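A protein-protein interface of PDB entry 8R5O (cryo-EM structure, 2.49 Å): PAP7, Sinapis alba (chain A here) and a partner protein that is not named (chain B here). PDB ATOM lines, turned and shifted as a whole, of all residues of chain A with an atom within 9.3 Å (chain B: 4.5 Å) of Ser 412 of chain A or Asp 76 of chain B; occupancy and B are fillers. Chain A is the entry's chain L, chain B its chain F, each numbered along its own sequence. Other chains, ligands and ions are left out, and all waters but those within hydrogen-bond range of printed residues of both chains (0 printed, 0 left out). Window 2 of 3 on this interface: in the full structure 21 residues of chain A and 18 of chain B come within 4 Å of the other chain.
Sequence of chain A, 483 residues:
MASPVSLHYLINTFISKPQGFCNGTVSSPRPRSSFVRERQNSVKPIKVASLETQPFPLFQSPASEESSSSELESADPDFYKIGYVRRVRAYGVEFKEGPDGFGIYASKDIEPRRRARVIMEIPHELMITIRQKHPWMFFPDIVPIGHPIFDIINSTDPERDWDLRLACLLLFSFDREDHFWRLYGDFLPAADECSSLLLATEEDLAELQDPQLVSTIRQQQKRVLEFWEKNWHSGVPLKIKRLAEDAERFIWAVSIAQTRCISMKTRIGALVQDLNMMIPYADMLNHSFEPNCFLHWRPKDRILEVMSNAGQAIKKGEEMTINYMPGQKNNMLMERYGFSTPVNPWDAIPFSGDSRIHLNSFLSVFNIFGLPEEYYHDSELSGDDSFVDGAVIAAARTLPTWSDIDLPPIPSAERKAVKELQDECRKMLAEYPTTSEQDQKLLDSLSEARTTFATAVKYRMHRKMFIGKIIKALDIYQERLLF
The side-chain carboxylate (OD1) of Asp 76 of chain B is in hydrogen-bond range of the side-chain hydroxyl (OG) of Ser 412 of chain A (2.8 Å).
SD of Met 79 of chain B touches CB of Pro 408 of chain A, at 3.6 Å. CG of Met 79 of chain B touches O of Pro 409 of chain A (3.9 Å). Asp 76 of chain B touches Ile 410 of chain A (OD1 to CG2, 3.4 Å). Ile 410 of chain A touches Glu 80 of chain B (CD1 to OE1, 3.5 Å). Leu 72 of chain B touches Pro 411 of chain A (CD1 to CB, 3.9 Å). CG of Pro 411 of chain A touches CG of Met 75 of chain B, 3.5 Å away. Asp 76 of chain B touches Pro 411 of chain A. CE of Met 75 of chain B touches C of Leu 482 of chain A (3.9 Å).
Ser 412 of chain A touches one residue of chain B. Asp 76 of chain B touches just these residues of chain A: Ile 410 (3.4 Å), Pro 411 (3.6 Å) and Ser 412 (2.8 Å). Of the printed residues of chain B, Pro 409 of chain A touches Met 79. Printed residues of chain B within 4 Å of Pro 408 of chain A: Met 79 (3.6 Å). Printed residues of chain B within 4 Å of Ile 410 of chain A: Asp 76 and Glu 80. Of the printed residues of chain A, Glu 80 of chain B touches Ile 410. The nearest residue of chain A that does not touch Asp 76 of chain B is Ala 413 of chain A (5.1 Å). The nearest printed residue of chain B that does not touch Pro 409 of chain A is Met 75 of chain B (6.0 Å).
Hydrophobic or aromatic side chains of chain A within 4 Å of the printed part of chain B: Pro 408, Ile 410 and Pro 411. Along chain A the printed residues that touch a printed residue of chain B span positions 408 to 482. Of the 9 printed residues of chain B, 5 touch a printed residue of chain A. Along chain B the printed residues that touch a printed residue of chain A span positions 72 to 80. Among the printed residues, no Asp or Glu carboxylate lies within 4 Å of a Lys or Arg side-chain nitrogen of the other chain.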
ATOM      1  N   ARG A 356       2.220  10.182 -11.060  1.00  0.00           N
ATOM      2  CA  ARG A 356       3.406  10.246 -11.903  1.00  0.00           C
ATOM      3  C   ARG A 356       3.261   9.292 -13.076  1.00  0.00           C
ATOM      4  O   ARG A 356       2.677   8.213 -12.944  1.00  0.00           O
ATOM      5  CB  ARG A 356       4.668   9.901 -11.110  1.00  0.00           C
ATOM      6  CG  ARG A 356       4.932  10.841  -9.953  1.00  0.00           C
ATOM      7  CD  ARG A 356       6.208  10.485  -9.226  1.00  0.00           C
ATOM      8  NE  ARG A 356       6.593  11.536  -8.294  1.00  0.00           N
ATOM      9  CZ  ARG A 356       7.376  12.560  -8.605  1.00  0.00           C
ATOM     10  NH1 ARG A 356       7.894  12.690  -9.815  1.00  0.00           N
ATOM     11  NH2 ARG A 356       7.647  13.475  -7.679  1.00  0.00           N
ATOM     12  N   PRO A 408       8.956  -1.912 -16.537  1.00  0.00           N
ATOM     13  CA  PRO A 408       7.912  -1.408 -17.433  1.00  0.00           C
ATOM     14  C   PRO A 408       6.725  -0.886 -16.646  1.00  0.00           C
ATOM     15  O   PRO A 408       6.484  -1.317 -15.509  1.00  0.00           O
ATOM     16  CB  PRO A 408       7.530  -2.642 -18.268  1.00  0.00           C
ATOM     17  CG  PRO A 408       8.376  -3.785 -17.751  1.00  0.00           C
ATOM     18  CD  PRO A 408       8.922  -3.377 -16.427  1.00  0.00           C
ATOM     19  N   PRO A 409       5.964   0.051 -17.210  1.00  0.00           N
ATOM     20  CA  PRO A 409       4.784   0.574 -16.513  1.00  0.00           C
ATOM     21  C   PRO A 409       3.527  -0.237 -16.788  1.00  0.00           C
ATOM     22  O   PRO A 409       3.268  -0.677 -17.910  1.00  0.00           O
ATOM     23  CB  PRO A 409       4.657   1.989 -17.089  1.00  0.00           C
ATOM     24  CG  PRO A 409       5.172   1.854 -18.480  1.00  0.00           C
ATOM     25  CD  PRO A 409       6.267   0.815 -18.434  1.00  0.00           C
ATOM     26  N   ILE A 410       2.741  -0.434 -15.737  1.00  0.00           N
ATOM     27  CA  ILE A 410       1.441  -1.104 -15.879  1.00  0.00           C
ATOM     28  C   ILE A 410       0.464  -0.154 -16.562  1.00  0.00           C
ATOM     29  O   ILE A 410       0.310   0.997 -16.114  1.00  0.00           O
ATOM     30  CB  ILE A 410       0.916  -1.544 -14.511  1.00  0.00           C
ATOM     31  CG1 ILE A 410       1.999  -2.298 -13.743  1.00  0.00           C
ATOM     32  CG2 ILE A 410      -0.310  -2.427 -14.668  1.00  0.00           C
ATOM     33  CD1 ILE A 410       1.589  -2.703 -12.349  1.00  0.00           C
ATOM     34  N   PRO A 411      -0.201  -0.570 -17.644  1.00  0.00           N
ATOM     35  CA  PRO A 411      -1.084   0.365 -18.365  1.00  0.00           C
ATOM     36  C   PRO A 411      -2.240   0.896 -17.534  1.00  0.00           C
ATOM     37  O   PRO A 411      -2.609   2.066 -17.679  1.00  0.00           O
ATOM     38  CB  PRO A 411      -1.581  -0.474 -19.550  1.00  0.00           C
ATOM     39  CG  PRO A 411      -0.583  -1.563 -19.693  1.00  0.00           C
ATOM     40  CD  PRO A 411      -0.128  -1.879 -18.308  1.00  0.00           C
ATOM     41  N   SER A 412      -2.825   0.070 -16.664  1.00  0.00           N
ATOM     42  CA  SER A 412      -3.983   0.518 -15.899  1.00  0.00           C
ATOM     43  C   SER A 412      -3.588   1.496 -14.801  1.00  0.00           C
ATOM     44  O   SER A 412      -4.375   2.381 -14.448  1.00  0.00           O
ATOM     45  CB  SER A 412      -4.721  -0.681 -15.308  1.00  0.00           C
ATOM     46  OG  SER A 412      -3.870  -1.435 -14.463  1.00  0.00           O
ATOM     47  N   ALA A 413      -2.383   1.352 -14.248  1.00  0.00           N
ATOM     48  CA  ALA A 413      -1.906   2.302 -13.251  1.00  0.00           C
ATOM     49  C   ALA A 413      -1.462   3.612 -13.884  1.00  0.00           C
ATOM     50  O   ALA A 413      -1.559   4.668 -13.248  1.00  0.00           O
ATOM     51  CB  ALA A 413      -0.758   1.687 -12.449  1.00  0.00           C
ATOM     52  N   GLU A 414      -0.974   3.566 -15.126  1.00  0.00           N
ATOM     53  CA  GLU A 414      -0.585   4.788 -15.818  1.00  0.00           C
ATOM     54  C   GLU A 414      -1.796   5.604 -16.242  1.00  0.00           C
ATOM     55  O   GLU A 414      -1.719   6.836 -16.310  1.00  0.00           O
ATOM     56  CB  GLU A 414       0.279   4.449 -17.030  1.00  0.00           C
ATOM     57  CG  GLU A 414       1.651   3.916 -16.676  1.00  0.00           C
ATOM     58  CD  GLU A 414       2.613   5.014 -16.276  1.00  0.00           C
ATOM     59  OE1 GLU A 414       2.798   5.958 -17.071  1.00  0.00           O
ATOM     60  OE2 GLU A 414       3.176   4.939 -15.165  1.00  0.00           O
ATOM     61  N   ARG A 415      -2.917   4.941 -16.536  1.00  0.00           N
ATOM     62  CA  ARG A 415      -4.124   5.665 -16.919  1.00  0.00           C
ATOM     63  C   ARG A 415      -4.688   6.460 -15.751  1.00  0.00           C
ATOM     64  O   ARG A 415      -5.219   7.560 -15.942  1.00  0.00           O
ATOM     65  CB  ARG A 415      -5.167   4.692 -17.466  1.00  0.00           C
ATOM     66  CG  ARG A 415      -4.814   4.152 -18.837  1.00  0.00           C
ATOM     67  CD  ARG A 415      -5.939   3.322 -19.423  1.00  0.00           C
ATOM     68  NE  ARG A 415      -6.023   3.508 -20.866  1.00  0.00           N
ATOM     69  CZ  ARG A 415      -6.814   4.392 -21.459  1.00  0.00           C
ATOM     70  NH1 ARG A 415      -7.634   5.160 -20.762  1.00  0.00           N
ATOM     71  NH2 ARG A 415      -6.783   4.504 -22.783  1.00  0.00           N
ATOM     72  N   LYS A 416      -4.592   5.917 -14.535  1.00  0.00           N
ATOM     73  CA  LYS A 416      -5.015   6.666 -13.358  1.00  0.00           C
ATOM     74  C   LYS A 416      -4.173   7.922 -13.176  1.00  0.00           C
ATOM     75  O   LYS A 416      -4.700   8.990 -12.844  1.00  0.00           O
ATOM     76  CB  LYS A 416      -4.933   5.780 -12.116  1.00  0.00           C
ATOM     77  CG  LYS A 416      -5.168   6.524 -10.814  1.00  0.00           C
ATOM     78  CD  LYS A 416      -4.984   5.616  -9.613  1.00  0.00           C
ATOM     79  CE  LYS A 416      -5.099   6.396  -8.314  1.00  0.00           C
ATOM     80  NZ  LYS A 416      -4.907   5.519  -7.126  1.00  0.00           N
ATOM     81  N   ALA A 417      -2.860   7.813 -13.389  1.00  0.00           N
ATOM     82  CA  ALA A 417      -1.988   8.977 -13.272  1.00  0.00           C
ATOM     83  C   ALA A 417      -2.288  10.004 -14.357  1.00  0.00           C
ATOM     84  O   ALA A 417      -2.386  11.203 -14.078  1.00  0.00           O
ATOM     85  CB  ALA A 417      -0.524   8.543 -13.333  1.00  0.00           C
ATOM     86  N   VAL A 418      -2.439   9.550 -15.603  1.00  0.00           N
ATOM     87  CA  VAL A 418      -2.747  10.465 -16.699  1.00  0.00           C
ATOM     88  C   VAL A 418      -4.072  11.170 -16.448  1.00  0.00           C
ATOM     89  O   VAL A 418      -4.199  12.382 -16.661  1.00  0.00           O
ATOM     90  CB  VAL A 418      -2.752   9.709 -18.041  1.00  0.00           C
ATOM     91  CG1 VAL A 418      -3.432  10.538 -19.118  1.00  0.00           C
ATOM     92  CG2 VAL A 418      -1.334   9.364 -18.456  1.00  0.00           C
ATOM     93  N   LYS A 419      -5.079  10.424 -15.990  1.00  0.00           N
ATOM     94  CA  LYS A 419      -6.372  11.025 -15.682  1.00  0.00           C
ATOM     95  C   LYS A 419      -6.252  12.056 -14.566  1.00  0.00           C
ATOM     96  O   LYS A 419      -6.841  13.140 -14.647  1.00  0.00           O
ATOM     97  CB  LYS A 419      -7.374   9.928 -15.312  1.00  0.00           C
ATOM     98  CG  LYS A 419      -8.278  10.239 -14.129  1.00  0.00           C
ATOM     99  CD  LYS A 419      -9.515  11.019 -14.538  1.00  0.00           C
ATOM    100  CE  LYS A 419     -10.470  11.172 -13.364  1.00  0.00           C
ATOM    101  NZ  LYS A 419     -11.656  12.007 -13.696  1.00  0.00           N
ATOM    102  N   GLU A 420      -5.487  11.741 -13.519  1.00  0.00           N
ATOM    103  CA  GLU A 420      -5.329  12.677 -12.411  1.00  0.00           C
ATOM    104  C   GLU A 420      -4.472  13.877 -12.798  1.00  0.00           C
ATOM    105  O   GLU A 420      -4.698  14.982 -12.294  1.00  0.00           O
ATOM    106  CB  GLU A 420      -4.737  11.959 -11.202  1.00  0.00           C
ATOM    107  CG  GLU A 420      -5.713  11.015 -10.517  1.00  0.00           C
ATOM    108  CD  GLU A 420      -5.044  10.105  -9.508  1.00  0.00           C
ATOM    109  OE1 GLU A 420      -3.842   9.811  -9.673  1.00  0.00           O
ATOM    110  OE2 GLU A 420      -5.721   9.683  -8.546  1.00  0.00           O
ATOM    111  N   GLN A 478      -1.339   8.255 -23.232  1.00  0.00           N
ATOM    112  CA  GLN A 478      -2.152   7.225 -22.595  1.00  0.00           C
ATOM    113  C   GLN A 478      -2.615   6.172 -23.593  1.00  0.00           C
ATOM    114  O   GLN A 478      -2.732   4.993 -23.241  1.00  0.00           O
ATOM    115  CB  GLN A 478      -3.353   7.871 -21.906  1.00  0.00           C
ATOM    116  CG  GLN A 478      -4.280   6.898 -21.211  1.00  0.00           C
ATOM    117  CD  GLN A 478      -5.534   7.569 -20.691  1.00  0.00           C
ATOM    118  OE1 GLN A 478      -5.656   7.841 -19.498  1.00  0.00           O
ATOM    119  NE2 GLN A 478      -6.475   7.837 -21.588  1.00  0.00           N
ATOM    120  N   LEU A 481       0.262   3.783 -25.256  1.00  0.00           N
ATOM    121  CA  LEU A 481       0.824   2.831 -24.307  1.00  0.00           C
ATOM    122  C   LEU A 481       0.127   1.477 -24.363  1.00  0.00           C
ATOM    123  O   LEU A 481       0.112   0.748 -23.363  1.00  0.00           O
ATOM    124  CB  LEU A 481       0.760   3.405 -22.892  1.00  0.00           C
ATOM    125  CG  LEU A 481       2.031   3.256 -22.060  1.00  0.00           C
ATOM    126  CD1 LEU A 481       3.189   3.936 -22.767  1.00  0.00           C
ATOM    127  CD2 LEU A 481       1.829   3.836 -20.673  1.00  0.00           C
ATOM    128  N   LEU A 482      -0.455   1.125 -25.506  1.00  0.00           N
ATOM    129  CA  LEU A 482      -1.164  -0.139 -25.658  1.00  0.00           C
ATOM    130  C   LEU A 482      -0.562  -0.975 -26.781  1.00  0.00           C
ATOM    131  O   LEU A 482      -1.269  -1.713 -27.462  1.00  0.00           O
ATOM    132  CB  LEU A 482      -2.648   0.107 -25.929  1.00  0.00           C
ATOM    133  CG  LEU A 482      -3.487   0.624 -24.761  1.00  0.00           C
ATOM    134  CD1 LEU A 482      -4.926   0.852 -25.193  1.00  0.00           C
ATOM    135  CD2 LEU A 482      -3.425  -0.352 -23.601  1.00  0.00           C
ATOM    136  N   LEU B  72      -6.223  -3.638 -23.311  1.00  0.00           N
ATOM    137  CA  LEU B  72      -5.896  -3.131 -21.982  1.00  0.00           C
ATOM    138  C   LEU B  72      -5.742  -4.263 -20.977  1.00  0.00           C
ATOM    139  O   LEU B  72      -4.784  -4.280 -20.196  1.00  0.00           O
ATOM    140  CB  LEU B  72      -6.966  -2.146 -21.515  1.00  0.00           C
ATOM    141  CG  LEU B  72      -6.751  -1.555 -20.120  1.00  0.00           C
ATOM    142  CD1 LEU B  72      -5.474  -0.730 -20.076  1.00  0.00           C
ATOM    143  CD2 LEU B  72      -7.944  -0.719 -19.696  1.00  0.00           C
ATOM    144  N   THR B  73      -6.669  -5.223 -20.979  1.00  0.00           N
ATOM    145  CA  THR B  73      -6.584  -6.317 -20.019  1.00  0.00           C
ATOM    146  C   THR B  73      -5.522  -7.339 -20.409  1.00  0.00           C
ATOM    147  O   THR B  73      -4.978  -8.020 -19.532  1.00  0.00           O
ATOM    148  CB  THR B  73      -7.948  -6.994 -19.850  1.00  0.00           C
ATOM    149  OG1 THR B  73      -7.851  -8.023 -18.857  1.00  0.00           O
ATOM    150  CG2 THR B  73      -8.427  -7.605 -21.153  1.00  0.00           C
ATOM    151  N   PHE B  74      -5.212  -7.464 -21.702  1.00  0.00           N
ATOM    152  CA  PHE B  74      -4.110  -8.330 -22.109  1.00  0.00           C
ATOM    153  C   PHE B  74      -2.763  -7.704 -21.769  1.00  0.00           C
ATOM    154  O   PHE B  74      -1.854  -8.395 -21.297  1.00  0.00           O
ATOM    155  CB  PHE B  74      -4.196  -8.634 -23.604  1.00  0.00           C
ATOM    156  CG  PHE B  74      -5.052  -9.821 -23.935  1.00  0.00           C
ATOM    157  CD1 PHE B  74      -6.395  -9.666 -24.222  1.00  0.00           C
ATOM    158  CD2 PHE B  74      -4.513 -11.095 -23.963  1.00  0.00           C
ATOM    159  CE1 PHE B  74      -7.184 -10.750 -24.527  1.00  0.00           C
ATOM    160  CE2 PHE B  74      -5.298 -12.184 -24.271  1.00  0.00           C
ATOM    161  CZ  PHE B  74      -6.636 -12.010 -24.553  1.00  0.00           C
ATOM    162  N   MET B  75      -2.615  -6.397 -22.001  1.00  0.00           N
ATOM    163  CA  MET B  75      -1.376  -5.716 -21.647  1.00  0.00           C
ATOM    164  C   MET B  75      -1.251  -5.496 -20.146  1.00  0.00           C
ATOM    165  O   MET B  75      -0.135  -5.325 -19.646  1.00  0.00           O
ATOM    166  CB  MET B  75      -1.274  -4.381 -22.388  1.00  0.00           C
ATOM    167  CG  MET B  75       0.099  -3.731 -22.327  1.00  0.00           C
ATOM    168  SD  MET B  75       1.376  -4.633 -23.220  1.00  0.00           S
ATOM    169  CE  MET B  75       1.259  -3.870 -24.834  1.00  0.00           C
ATOM    170  N   ASP B  76      -2.367  -5.491 -19.415  1.00  0.00           N
ATOM    171  CA  ASP B  76      -2.295  -5.464 -17.958  1.00  0.00           C
ATOM    172  C   ASP B  76      -1.688  -6.753 -17.422  1.00  0.00           C
ATOM    173  O   ASP B  76      -0.794  -6.725 -16.568  1.00  0.00           O
ATOM    174  CB  ASP B  76      -3.684  -5.242 -17.362  1.00  0.00           C
ATOM    175  CG  ASP B  76      -3.960  -3.788 -17.052  1.00  0.00           C
ATOM    176  OD1 ASP B  76      -3.029  -3.090 -16.601  1.00  0.00           O
ATOM    177  OD2 ASP B  76      -5.109  -3.345 -17.255  1.00  0.00           O
ATOM    178  N   GLU B  77      -2.166  -7.897 -17.913  1.00  0.00           N
ATOM    179  CA  GLU B  77      -1.636  -9.179 -17.462  1.00  0.00           C
ATOM    180  C   GLU B  77      -0.191  -9.368 -17.904  1.00  0.00           C
ATOM    181  O   GLU B  77       0.634  -9.877 -17.138  1.00  0.00           O
ATOM    182  CB  GLU B  77      -2.511 -10.318 -17.981  1.00  0.00           C
ATOM    183  CG  GLU B  77      -2.069 -11.693 -17.521  1.00  0.00           C
ATOM    184  CD  GLU B  77      -2.119 -11.845 -16.015  1.00  0.00           C
ATOM    185  OE1 GLU B  77      -3.023 -11.257 -15.386  1.00  0.00           O
ATOM    186  OE2 GLU B  77      -1.251 -12.548 -15.459  1.00  0.00           O
ATOM    187  N   LEU B  78       0.131  -8.966 -19.134  1.00  0.00           N
ATOM    188  CA  LEU B  78       1.483  -9.159 -19.648  1.00  0.00           C
ATOM    189  C   LEU B  78       2.495  -8.345 -18.854  1.00  0.00           C
ATOM    190  O   LEU B  78       3.544  -8.858 -18.451  1.00  0.00           O
ATOM    191  CB  LEU B  78       1.533  -8.792 -21.133  1.00  0.00           C
ATOM    192  CG  LEU B  78       2.838  -9.075 -21.879  1.00  0.00           C
ATOM    193  CD1 LEU B  78       2.541  -9.660 -23.245  1.00  0.00           C
ATOM    194  CD2 LEU B  78       3.680  -7.815 -22.015  1.00  0.00           C
ATOM    195  N   MET B  79       2.194  -7.067 -18.613  1.00  0.00           N
ATOM    196  CA  MET B  79       3.135  -6.214 -17.898  1.00  0.00           C
ATOM    197  C   MET B  79       3.177  -6.510 -16.405  1.00  0.00           C
ATOM    198  O   MET B  79       4.139  -6.115 -15.739  1.00  0.00           O
ATOM    199  CB  MET B  79       2.800  -4.741 -18.134  1.00  0.00           C
ATOM    200  CG  MET B  79       3.282  -4.220 -19.475  1.00  0.00           C
ATOM    201  SD  MET B  79       5.000  -4.679 -19.773  1.00  0.00           S
ATOM    202  CE  MET B  79       5.308  -3.881 -21.346  1.00  0.00           C
ATOM    203  N   GLU B  80       2.168  -7.192 -15.864  1.00  0.00           N
ATOM    204  CA  GLU B  80       2.225  -7.618 -14.472  1.00  0.00           C
ATOM    205  C   GLU B  80       3.061  -8.875 -14.276  1.00  0.00           C
ATOM    206  O   GLU B  80       3.394  -9.204 -13.133  1.00  0.00           O
ATOM    207  CB  GLU B  80       0.816  -7.853 -13.920  1.00  0.00           C
ATOM    208  CG  GLU B  80       0.065  -6.583 -13.537  1.00  0.00           C
ATOM    209  CD  GLU B  80       0.478  -6.025 -12.183  1.00  0.00           C
ATOM    210  OE1 GLU B  80       1.661  -6.149 -11.808  1.00  0.00           O
ATOM    211  OE2 GLU B  80      -0.392  -5.457 -11.489  1.00  0.00           O
